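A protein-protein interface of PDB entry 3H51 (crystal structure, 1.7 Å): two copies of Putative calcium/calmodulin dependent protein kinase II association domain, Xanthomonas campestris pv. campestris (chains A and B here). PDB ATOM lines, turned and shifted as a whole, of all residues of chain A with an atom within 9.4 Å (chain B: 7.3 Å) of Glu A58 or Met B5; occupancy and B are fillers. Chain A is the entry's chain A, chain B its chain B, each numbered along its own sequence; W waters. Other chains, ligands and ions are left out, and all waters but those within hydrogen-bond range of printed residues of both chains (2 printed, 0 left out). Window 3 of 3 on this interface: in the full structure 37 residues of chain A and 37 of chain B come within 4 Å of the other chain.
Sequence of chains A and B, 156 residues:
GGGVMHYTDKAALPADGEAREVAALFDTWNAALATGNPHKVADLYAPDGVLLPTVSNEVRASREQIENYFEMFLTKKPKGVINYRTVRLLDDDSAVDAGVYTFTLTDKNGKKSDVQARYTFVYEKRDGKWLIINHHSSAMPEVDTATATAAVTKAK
Water W1 bridges OG of Ser A56 (2.5 Å) and OE1 of Glu B142 (3.2 Å). Water W2 lies within hydrogen-bond range of the backbone carbonyl oxygen of Asn A57, the guanidinium group of Arg B118 and the backbone carbonyl oxygen of Ser A56.
No position is printed for both chains. Of the 19 pairs that touch across the chains among the printed residues, none has its exchanged pair printed and touching as well.
Printed residues of chain A that touch a printed residue of chain B: Leu A52, Pro A53, Thr A54, Val A55, Ser A56, Asn A57, Glu A58 and Val A59. Hydrophobic or aromatic side chains of chain A within 4 Å of the printed part of chain B: Leu A52, Pro A53 and Val A59. Hydrophobic or aromatic side chains of chain B within 4 Å of the printed part of chain A: Val B4, Met B5, His B6, Tyr B7, Val B100, Met B140 and Pro B141.
NH1 of Arg B118 sits at hydrogen-bond distance from O of Pro A53, at 2.7 Å. N of Val A59 is in hydrogen-bond range of OH of Tyr B7 (2.9 Å). The backbone nitrogen (N) of Pro B141 sits close to the side-chain amide oxygen (OD1) of Asn A57 (3.2 Å). N of Asn A57 is in hydrogen-bond range of OE1 of Glu B142, 2.6 Å away. The backbone carbonyl oxygen of Met B5 sits at hydrogen-bond distance from the side-chain amide nitrogen of Asn A57 (3.1 Å).
Among the printed residues, merely in contact across the chains: Thr A54 with Pro B141 (3.2 Å), Asn A57 with Tyr B7 (3.4 Å), Asn A57 with Val B4 (3.4 Å), Ser A56 with Glu B142 (3.5 Å), Ser A56 with Arg B118 (3.5 Å), Glu A58 with Tyr B7 (3.6 Å), Leu A52 with Arg B118 (3.6 Å), Ser A56 with Pro B141 (3.6 Å), Asn A57 with Met B140 (3.6 Å), Val A59 with Val B100 (3.7 Å), Asn A57 with His B6 (3.7 Å), Val A55 with Glu B142 (3.7 Å), Glu A58 with Met B5 (3.8 Å) and Val A55 with Pro B141 (3.9 Å).
Of chain B, only Met B5 and Tyr B7 come within 4 Å of Glu A58. Of chain A, only Asn A57 (3.1 Å) and Glu A58 (3.8 Å) come within 4 Å of Met B5. Val B4 touches just one residue of chain A: Asn A57 (3.4 Å). His B6 touches one residue of chain A. Of the printed residues of chain B, Pro A53 touches Arg B118 (2.7 Å). Of the printed residues of chain A, Tyr B7 touches Asn A57, Glu A58 and Val A59. Of the printed residues of chain B, Thr A54 touches Pro B141 (3.2 Å). Of the printed residues of chain A, Glu B142 touches Val A55, Ser A56 and Asn A57. Ser A62 touches none of the printed residues of chain B. Tyr A69 touches none of the printed residues of chain B. The nearest residue of chain B that does not touch Glu A58 is Glu B142 (4.5 Å). The nearest residue of chain A that does not touch Met B5 is Val A59 (5.4 Å).
The backbone carbonyl oxygen of Tyr B7 lies within hydrogen-bond range of the side-chain amide nitrogen of Gln B116. OH of Tyr A69 sits at hydrogen-bond distance from N of Thr A54 (3.5 Å). OG of Ser A56 sits close to N of Glu A58. The guanidinium group (NH2) of Arg A60 is in salt-bridge range of the side-chain carboxylate (OE1) of Glu A58 (3.8 Å). The backbone carbonyl oxygen (O) of Gln B116 sits close to the backbone NH (N) of Met B140. NE2 of Gln A65 lies within hydrogen-bond range of OE2 of Glu A58 (2.7 Å).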
ATOM      1  N   VAL A  50     -25.022  -5.363 -12.289  1.00  0.00           N
ATOM      2  CA  VAL A  50     -24.170  -4.445 -11.506  1.00  0.00           C
ATOM      3  C   VAL A  50     -24.224  -3.064 -12.192  1.00  0.00           C
ATOM      4  O   VAL A  50     -23.945  -2.938 -13.365  1.00  0.00           O
ATOM      5  CB  VAL A  50     -22.701  -4.969 -11.357  1.00  0.00           C
ATOM      6  CG1 VAL A  50     -21.819  -4.039 -10.530  1.00  0.00           C
ATOM      7  CG2 VAL A  50     -22.644  -6.472 -10.834  1.00  0.00           C
ATOM      8  N   LEU A  51     -24.614  -2.055 -11.422  1.00  0.00           N
ATOM      9  CA  LEU A  51     -24.657  -0.653 -11.829  1.00  0.00           C
ATOM     10  C   LEU A  51     -23.571   0.199 -11.105  1.00  0.00           C
ATOM     11  O   LEU A  51     -23.475   0.210  -9.865  1.00  0.00           O
ATOM     12  CB  LEU A  51     -26.058  -0.101 -11.535  1.00  0.00           C
ATOM     13  CG  LEU A  51     -26.325   1.397 -11.684  1.00  0.00           C
ATOM     14  CD1 LEU A  51     -26.188   1.840 -13.174  1.00  0.00           C
ATOM     15  CD2 LEU A  51     -27.703   1.865 -11.092  1.00  0.00           C
ATOM     16  N   LEU A  52     -22.785   0.913 -11.873  1.00  0.00           N
ATOM     17  CA  LEU A  52     -21.727   1.793 -11.417  1.00  0.00           C
ATOM     18  C   LEU A  52     -22.137   3.165 -11.962  1.00  0.00           C
ATOM     19  O   LEU A  52     -21.836   3.503 -13.099  1.00  0.00           O
ATOM     20  CB  LEU A  52     -20.369   1.303 -11.941  1.00  0.00           C
ATOM     21  CG  LEU A  52     -20.084  -0.189 -11.658  1.00  0.00           C
ATOM     22  CD1 LEU A  52     -20.412  -1.111 -12.808  1.00  0.00           C
ATOM     23  CD2 LEU A  52     -18.655  -0.350 -11.268  1.00  0.00           C
ATOM     24  N   PRO A  53     -22.980   3.862 -11.169  1.00  0.00           N
ATOM     25  CA  PRO A  53     -23.783   4.963 -11.666  1.00  0.00           C
ATOM     26  C   PRO A  53     -23.096   6.315 -11.735  1.00  0.00           C
ATOM     27  O   PRO A  53     -21.997   6.505 -11.171  1.00  0.00           O
ATOM     28  CB  PRO A  53     -24.930   4.997 -10.677  1.00  0.00           C
ATOM     29  CG  PRO A  53     -24.343   4.619  -9.452  1.00  0.00           C
ATOM     30  CD  PRO A  53     -23.318   3.564  -9.767  1.00  0.00           C
ATOM     31  N   THR A  54     -23.689   7.249 -12.473  1.00  0.00           N
ATOM     32  CA  THR A  54     -23.082   8.546 -12.684  1.00  0.00           C
ATOM     33  C   THR A  54     -22.799   9.308 -11.403  1.00  0.00           C
ATOM     34  O   THR A  54     -21.703   9.880 -11.257  1.00  0.00           O
ATOM     35  CB  THR A  54     -23.943   9.423 -13.643  1.00  0.00           C
ATOM     36  OG1 THR A  54     -24.544   8.619 -14.676  1.00  0.00           O
ATOM     37  CG2 THR A  54     -23.065  10.439 -14.348  1.00  0.00           C
ATOM     38  N   VAL A  55     -23.767   9.359 -10.481  1.00  0.00           N
ATOM     39  CA  VAL A  55     -23.639  10.303  -9.356  1.00  0.00           C
ATOM     40  C   VAL A  55     -23.471   9.693  -7.946  1.00  0.00           C
ATOM     41  O   VAL A  55     -23.542  10.409  -6.958  1.00  0.00           O
ATOM     42  CB  VAL A  55     -24.813  11.330  -9.348  1.00  0.00           C
ATOM     43  CG1 VAL A  55     -24.914  12.013 -10.711  1.00  0.00           C
ATOM     44  CG2 VAL A  55     -26.126  10.671  -9.002  1.00  0.00           C
ATOM     45  N   SER A  56     -23.225   8.394  -7.856  1.00  0.00           N
ATOM     46  CA  SER A  56     -23.033   7.771  -6.553  1.00  0.00           C
ATOM     47  C   SER A  56     -21.774   6.942  -6.495  1.00  0.00           C
ATOM     48  O   SER A  56     -21.519   6.195  -7.425  1.00  0.00           O
ATOM     49  CB  SER A  56     -24.216   6.817  -6.216  1.00  0.00           C
ATOM     50  OG  SER A  56     -24.142   6.359  -4.853  1.00  0.00           O
ATOM     51  N   ASN A  57     -21.046   7.015  -5.366  1.00  0.00           N
ATOM     52  CA  ASN A  57     -19.912   6.129  -5.185  1.00  0.00           C
ATOM     53  C   ASN A  57     -20.329   4.690  -4.955  1.00  0.00           C
ATOM     54  O   ASN A  57     -19.501   3.792  -5.141  1.00  0.00           O
ATOM     55  CB  ASN A  57     -19.040   6.520  -3.996  1.00  0.00           C
ATOM     56  CG  ASN A  57     -18.205   7.766  -4.232  1.00  0.00           C
ATOM     57  OD1 ASN A  57     -18.288   8.414  -5.269  1.00  0.00           O
ATOM     58  ND2 ASN A  57     -17.392   8.114  -3.228  1.00  0.00           N
ATOM     59  N   GLU A  58     -21.566   4.455  -4.522  1.00  0.00           N
ATOM     60  CA  GLU A  58     -21.975   3.127  -4.076  1.00  0.00           C
ATOM     61  C   GLU A  58     -22.350   2.303  -5.317  1.00  0.00           C
ATOM     62  O   GLU A  58     -23.279   2.619  -6.063  1.00  0.00           O
ATOM     63  CB  GLU A  58     -23.171   3.223  -3.155  1.00  0.00           C
ATOM     64  CG  GLU A  58     -23.653   1.843  -2.689  1.00  0.00           C
ATOM     65  CD  GLU A  58     -24.947   1.935  -1.907  1.00  0.00           C
ATOM     66  OE1 GLU A  58     -25.408   3.068  -1.603  1.00  0.00           O
ATOM     67  OE2 GLU A  58     -25.514   0.864  -1.619  1.00  0.00           O
ATOM     68  N   VAL A  59     -21.565   1.256  -5.561  1.00  0.00           N
ATOM     69  CA  VAL A  59     -21.848   0.310  -6.636  1.00  0.00           C
ATOM     70  C   VAL A  59     -23.082  -0.508  -6.238  1.00  0.00           C
ATOM     71  O   VAL A  59     -23.243  -0.902  -5.090  1.00  0.00           O
ATOM     72  CB  VAL A  59     -20.667  -0.628  -6.865  1.00  0.00           C
ATOM     73  CG1 VAL A  59     -21.050  -1.747  -7.877  1.00  0.00           C
ATOM     74  CG2 VAL A  59     -19.384   0.206  -7.317  1.00  0.00           C
ATOM     75  N   ARG A  60     -24.014  -0.651  -7.166  1.00  0.00           N
ATOM     76  CA  ARG A  60     -25.302  -1.266  -6.877  1.00  0.00           C
ATOM     77  C   ARG A  60     -25.346  -2.662  -7.482  1.00  0.00           C
ATOM     78  O   ARG A  60     -25.262  -2.820  -8.719  1.00  0.00           O
ATOM     79  CB  ARG A  60     -26.448  -0.421  -7.428  1.00  0.00           C
ATOM     80  CG  ARG A  60     -26.367   1.077  -7.154  1.00  0.00           C
ATOM     81  CD  ARG A  60     -26.247   1.394  -5.691  1.00  0.00           C
ATOM     82  NE  ARG A  60     -26.073   2.830  -5.421  1.00  0.00           N
ATOM     83  CZ  ARG A  60     -26.996   3.619  -4.904  1.00  0.00           C
ATOM     84  NH1 ARG A  60     -28.221   3.192  -4.673  1.00  0.00           N
ATOM     85  NH2 ARG A  60     -26.716   4.888  -4.674  1.00  0.00           N
ATOM     86  N   ALA A  61     -25.430  -3.669  -6.617  1.00  0.00           N
ATOM     87  CA  ALA A  61     -25.345  -5.073  -7.075  1.00  0.00           C
ATOM     88  C   ALA A  61     -26.526  -5.903  -6.576  1.00  0.00           C
ATOM     89  O   ALA A  61     -26.413  -7.100  -6.467  1.00  0.00           O
ATOM     90  CB  ALA A  61     -23.969  -5.709  -6.676  1.00  0.00           C
ATOM     91  N   SER A  62     -27.646  -5.261  -6.240  1.00  0.00           N
ATOM     92  CA  SER A  62     -28.900  -5.943  -6.006  1.00  0.00           C
ATOM     93  C   SER A  62     -30.012  -5.117  -6.620  1.00  0.00           C
ATOM     94  O   SER A  62     -29.842  -3.910  -6.824  1.00  0.00           O
ATOM     95  CB  SER A  62     -29.160  -6.119  -4.510  1.00  0.00           C
ATOM     96  OG  SER A  62     -29.425  -4.877  -3.860  1.00  0.00           O
ATOM     97  N   GLU A  64     -32.614  -4.114  -5.127  1.00  0.00           N
ATOM     98  CA  GLU A  64     -32.969  -3.090  -4.132  1.00  0.00           C
ATOM     99  C   GLU A  64     -32.036  -1.889  -4.251  1.00  0.00           C
ATOM    100  O   GLU A  64     -32.477  -0.745  -4.218  1.00  0.00           O
ATOM    101  CB  GLU A  64     -32.946  -3.648  -2.677  1.00  0.00           C
ATOM    102  CG  GLU A  64     -33.442  -2.619  -1.629  1.00  0.00           C
ATOM    103  CD  GLU A  64     -33.468  -3.104  -0.172  1.00  0.00           C
ATOM    104  OE1 GLU A  64     -32.501  -3.744   0.296  1.00  0.00           O
ATOM    105  OE2 GLU A  64     -34.451  -2.788   0.528  1.00  0.00           O
ATOM    106  N   GLN A  65     -30.740  -2.149  -4.404  1.00  0.00           N
ATOM    107  CA  GLN A  65     -29.780  -1.070  -4.509  1.00  0.00           C
ATOM    108  C   GLN A  65     -29.921  -0.304  -5.832  1.00  0.00           C
ATOM    109  O   GLN A  65     -29.725   0.927  -5.872  1.00  0.00           O
ATOM    110  CB  GLN A  65     -28.399  -1.640  -4.406  1.00  0.00           C
ATOM    111  CG  GLN A  65     -27.945  -2.036  -3.034  1.00  0.00           C
ATOM    112  CD  GLN A  65     -26.429  -2.418  -3.099  1.00  0.00           C
ATOM    113  OE1 GLN A  65     -26.020  -3.250  -3.911  1.00  0.00           O
ATOM    114  NE2 GLN A  65     -25.601  -1.757  -2.276  1.00  0.00           N
ATOM    115  N   ILE A  66     -30.220  -1.008  -6.905  1.00  0.00           N
ATOM    116  CA  ILE A  66     -30.531  -0.352  -8.205  1.00  0.00           C
ATOM    117  C   ILE A  66     -31.767   0.541  -8.088  1.00  0.00           C
ATOM    118  O   ILE A  66     -31.743   1.693  -8.489  1.00  0.00           O
ATOM    119  CB  ILE A  66     -30.610  -1.367  -9.369  1.00  0.00           C
ATOM    120  CG1 ILE A  66     -29.220  -1.976  -9.541  1.00  0.00           C
ATOM    121  CG2 ILE A  66     -31.114  -0.727 -10.651  1.00  0.00           C
ATOM    122  CD1 ILE A  66     -28.993  -3.133 -10.520  1.00  0.00           C
ATOM    123  N   ASN A  68     -32.970   1.894  -5.465  1.00  0.00           N
ATOM    124  CA  ASN A  68     -32.621   3.015  -4.613  1.00  0.00           C
ATOM    125  C   ASN A  68     -31.976   4.151  -5.431  1.00  0.00           C
ATOM    126  O   ASN A  68     -32.323   5.334  -5.277  1.00  0.00           O
ATOM    127  CB  ASN A  68     -31.712   2.551  -3.476  1.00  0.00           C
ATOM    128  CG  ASN A  68     -31.186   3.733  -2.644  1.00  0.00           C
ATOM    129  OD1 ASN A  68     -30.150   4.321  -2.972  1.00  0.00           O
ATOM    130  ND2 ASN A  68     -31.953   4.132  -1.607  1.00  0.00           N
ATOM    131  N   TYR A  69     -31.058   3.805  -6.339  1.00  0.00           N
ATOM    132  CA  TYR A  69     -30.456   4.814  -7.177  1.00  0.00           C
ATOM    133  C   TYR A  69     -31.465   5.567  -8.038  1.00  0.00           C
ATOM    134  O   TYR A  69     -31.449   6.809  -8.102  1.00  0.00           O
ATOM    135  CB  TYR A  69     -29.393   4.226  -8.103  1.00  0.00           C
ATOM    136  CG  TYR A  69     -28.675   5.289  -8.904  1.00  0.00           C
ATOM    137  CD1 TYR A  69     -27.683   6.059  -8.324  1.00  0.00           C
ATOM    138  CD2 TYR A  69     -29.031   5.567 -10.224  1.00  0.00           C
ATOM    139  CE1 TYR A  69     -27.025   7.031  -9.058  1.00  0.00           C
ATOM    140  CE2 TYR A  69     -28.406   6.551 -10.958  1.00  0.00           C
ATOM    141  CZ  TYR A  69     -27.365   7.256 -10.386  1.00  0.00           C
ATOM    142  OH  TYR A  69     -26.721   8.235 -11.096  1.00  0.00           O
ATOM    143  N   MET A  72     -33.837   8.308  -6.645  1.00  0.00           N
ATOM    144  CA  MET A  72     -33.275   9.659  -6.663  1.00  0.00           C
ATOM    145  C   MET A  72     -33.193  10.154  -8.091  1.00  0.00           C
ATOM    146  O   MET A  72     -33.773  11.182  -8.418  1.00  0.00           O
ATOM    147  CB  MET A  72     -31.887   9.693  -6.007  1.00  0.00           C
ATOM    148  CG  MET A  72     -31.120  11.026  -6.166  1.00  0.00           C
ATOM    149  SD  MET A  72     -29.985  11.162  -7.769  1.00  0.00           S
ATOM    150  CE  MET A  72     -29.242   9.332  -7.828  1.00  0.00           C
ATOM    151  N   HIS A 135     -24.007  -1.968 -16.087  1.00  0.00           N
ATOM    152  CA  HIS A 135     -24.165  -0.572 -16.621  1.00  0.00           C
ATOM    153  C   HIS A 135     -23.193   0.317 -15.829  1.00  0.00           C
ATOM    154  O   HIS A 135     -23.271   0.391 -14.585  1.00  0.00           O
ATOM    155  CB  HIS A 135     -25.620  -0.132 -16.390  1.00  0.00           C
ATOM    156  CG  HIS A 135     -25.938   1.274 -16.812  1.00  0.00           C
ATOM    157  ND1 HIS A 135     -27.145   1.873 -16.480  1.00  0.00           N
ATOM    158  CD2 HIS A 135     -25.274   2.155 -17.604  1.00  0.00           C
ATOM    159  CE1 HIS A 135     -27.178   3.081 -17.016  1.00  0.00           C
ATOM    160  NE2 HIS A 135     -26.048   3.286 -17.682  1.00  0.00           N
ATOM    161  N   VAL B   4     -21.795   8.772   2.337  1.00  0.00           N
ATOM    162  CA  VAL B   4     -20.919   8.425   1.134  1.00  0.00           C
ATOM    163  C   VAL B   4     -20.121   7.120   1.281  1.00  0.00           C
ATOM    164  O   VAL B   4     -19.393   6.924   2.268  1.00  0.00           O
ATOM    165  CB  VAL B   4     -19.872   9.511   0.800  1.00  0.00           C
ATOM    166  CG1 VAL B   4     -18.984   9.049  -0.380  1.00  0.00           C
ATOM    167  CG2 VAL B   4     -20.528  10.826   0.502  1.00  0.00           C
ATOM    168  N   MET B   5     -20.210   6.266   0.258  1.00  0.00           N
ATOM    169  CA  MET B   5     -19.537   4.968   0.258  1.00  0.00           C
ATOM    170  C   MET B   5     -18.065   5.183  -0.087  1.00  0.00           C
ATOM    171  O   MET B   5     -17.705   5.910  -1.024  1.00  0.00           O
ATOM    172  CB  MET B   5     -20.229   3.987  -0.711  1.00  0.00           C
ATOM    173  CG  MET B   5     -19.795   2.500  -0.632  1.00  0.00           C
ATOM    174  SD  MET B   5     -20.227   1.624   1.053  1.00  0.00           S
ATOM    175  CE  MET B   5     -22.129   1.265   0.780  1.00  0.00           C
ATOM    176  N   HIS B   6     -17.206   4.566   0.716  1.00  0.00           N
ATOM    177  CA  HIS B   6     -15.821   4.381   0.323  1.00  0.00           C
ATOM    178  C   HIS B   6     -15.470   2.896   0.395  1.00  0.00           C
ATOM    179  O   HIS B   6     -16.102   2.126   1.110  1.00  0.00           O
ATOM    180  CB  HIS B   6     -14.878   5.291   1.131  1.00  0.00           C
ATOM    181  CG  HIS B   6     -15.044   6.747   0.794  1.00  0.00           C
ATOM    182  ND1 HIS B   6     -14.739   7.262  -0.451  1.00  0.00           N
ATOM    183  CD2 HIS B   6     -15.545   7.780   1.514  1.00  0.00           C
ATOM    184  CE1 HIS B   6     -15.001   8.556  -0.470  1.00  0.00           C
ATOM    185  NE2 HIS B   6     -15.498   8.895   0.709  1.00  0.00           N
ATOM    186  N   TYR B   7     -14.521   2.495  -0.437  1.00  0.00           N
ATOM    187  CA  TYR B   7     -14.079   1.102  -0.500  1.00  0.00           C
ATOM    188  C   TYR B   7     -12.633   1.132  -0.064  1.00  0.00           C
ATOM    189  O   TYR B   7     -11.780   1.644  -0.771  1.00  0.00           O
ATOM    190  CB  TYR B   7     -14.269   0.570  -1.934  1.00  0.00           C
ATOM    191  CG  TYR B   7     -15.723   0.535  -2.336  1.00  0.00           C
ATOM    192  CD1 TYR B   7     -16.342   1.658  -2.917  1.00  0.00           C
ATOM    193  CD2 TYR B   7     -16.496  -0.611  -2.138  1.00  0.00           C
ATOM    194  CE1 TYR B   7     -17.692   1.614  -3.281  1.00  0.00           C
ATOM    195  CE2 TYR B   7     -17.844  -0.640  -2.487  1.00  0.00           C
ATOM    196  CZ  TYR B   7     -18.417   0.455  -3.078  1.00  0.00           C
ATOM    197  OH  TYR B   7     -19.753   0.415  -3.428  1.00  0.00           O
ATOM    198  N   VAL B 100     -14.421  -1.593  -7.994  1.00  0.00           N
ATOM    199  CA  VAL B 100     -13.733  -0.407  -7.594  1.00  0.00           C
ATOM    200  C   VAL B 100     -12.267  -0.756  -7.432  1.00  0.00           C
ATOM    201  O   VAL B 100     -11.907  -1.794  -6.853  1.00  0.00           O
ATOM    202  CB  VAL B 100     -14.336   0.148  -6.270  1.00  0.00           C
ATOM    203  CG1 VAL B 100     -13.531   1.355  -5.761  1.00  0.00           C
ATOM    204  CG2 VAL B 100     -15.817   0.496  -6.500  1.00  0.00           C
ATOM    205  N   GLN B 116      -8.947   6.640  -6.585  1.00  0.00           N
ATOM    206  CA  GLN B 116      -9.872   5.536  -6.615  1.00  0.00           C
ATOM    207  C   GLN B 116     -10.872   5.714  -7.768  1.00  0.00           C
ATOM    208  O   GLN B 116     -11.278   6.844  -8.105  1.00  0.00           O
ATOM    209  CB  GLN B 116     -10.600   5.415  -5.277  1.00  0.00           C
ATOM    210  CG  GLN B 116     -11.446   4.198  -5.186  1.00  0.00           C
ATOM    211  CD  GLN B 116     -11.874   3.910  -3.795  1.00  0.00           C
ATOM    212  OE1 GLN B 116     -12.578   4.729  -3.171  1.00  0.00           O
ATOM    213  NE2 GLN B 116     -11.474   2.756  -3.283  1.00  0.00           N
ATOM    214  N   ARG B 118     -14.151   3.540 -10.340  1.00  0.00           N
ATOM    215  CA  ARG B 118     -14.929   2.346 -10.627  1.00  0.00           C
ATOM    216  C   ARG B 118     -14.360   1.768 -11.948  1.00  0.00           C
ATOM    217  O   ARG B 118     -13.855   2.527 -12.781  1.00  0.00           O
ATOM    218  CB  ARG B 118     -16.410   2.675 -10.851  1.00  0.00           C
ATOM    219  CG  ARG B 118     -17.112   3.314  -9.656  1.00  0.00           C
ATOM    220  CD  ARG B 118     -17.022   4.864  -9.573  1.00  0.00           C
ATOM    221  NE  ARG B 118     -17.492   5.518 -10.803  1.00  0.00           N
ATOM    222  CZ  ARG B 118     -18.781   5.688 -11.131  1.00  0.00           C
ATOM    223  NH1 ARG B 118     -19.757   5.273 -10.311  1.00  0.00           N
ATOM    224  NH2 ARG B 118     -19.084   6.269 -12.281  1.00  0.00           N
ATOM    225  N   MET B 140     -14.306   8.298  -8.739  1.00  0.00           N
ATOM    226  CA  MET B 140     -15.416   8.255  -7.802  1.00  0.00           C
ATOM    227  C   MET B 140     -16.135   9.584  -7.909  1.00  0.00           C
ATOM    228  O   MET B 140     -15.491  10.642  -7.832  1.00  0.00           O
ATOM    229  CB  MET B 140     -14.898   8.027  -6.385  1.00  0.00           C
ATOM    230  CG  MET B 140     -14.007   6.834  -6.286  1.00  0.00           C
ATOM    231  SD  MET B 140     -14.926   5.171  -6.683  1.00  0.00           S
ATOM    232  CE  MET B 140     -15.931   5.012  -4.984  1.00  0.00           C
ATOM    233  N   PRO B 141     -17.458   9.550  -8.185  1.00  0.00           N
ATOM    234  CA  PRO B 141     -18.135  10.816  -8.397  1.00  0.00           C
ATOM    235  C   PRO B 141     -18.371  11.719  -7.175  1.00  0.00           C
ATOM    236  O   PRO B 141     -18.597  12.927  -7.335  1.00  0.00           O
ATOM    237  CB  PRO B 141     -19.467  10.397  -9.026  1.00  0.00           C
ATOM    238  CG  PRO B 141     -19.671   9.029  -8.621  1.00  0.00           C
ATOM    239  CD  PRO B 141     -18.349   8.402  -8.421  1.00  0.00           C
ATOM    240  N   GLU B 142     -18.364  11.130  -5.999  1.00  0.00           N
ATOM    241  CA  GLU B 142     -18.499  11.848  -4.744  1.00  0.00           C
ATOM    242  C   GLU B 142     -17.087  11.972  -4.125  1.00  0.00           C
ATOM    243  O   GLU B 142     -16.432  10.983  -3.711  1.00  0.00           O
ATOM    244  CB  GLU B 142     -19.453  11.111  -3.826  1.00  0.00           C
ATOM    245  CG  GLU B 142     -20.850  10.884  -4.393  1.00  0.00           C
ATOM    246  CD  GLU B 142     -21.727  10.048  -3.472  1.00  0.00           C
ATOM    247  OE1 GLU B 142     -21.664   8.794  -3.525  1.00  0.00           O
ATOM    248  OE2 GLU B 142     -22.486  10.649  -2.657  1.00  0.00           O
HETATM  249  O   HOH W   1     -24.832   8.249  -3.361  1.00  0.00           O
HETATM  250  O   HOH W   2     -20.072   3.717  -7.936  1.00  0.00           O
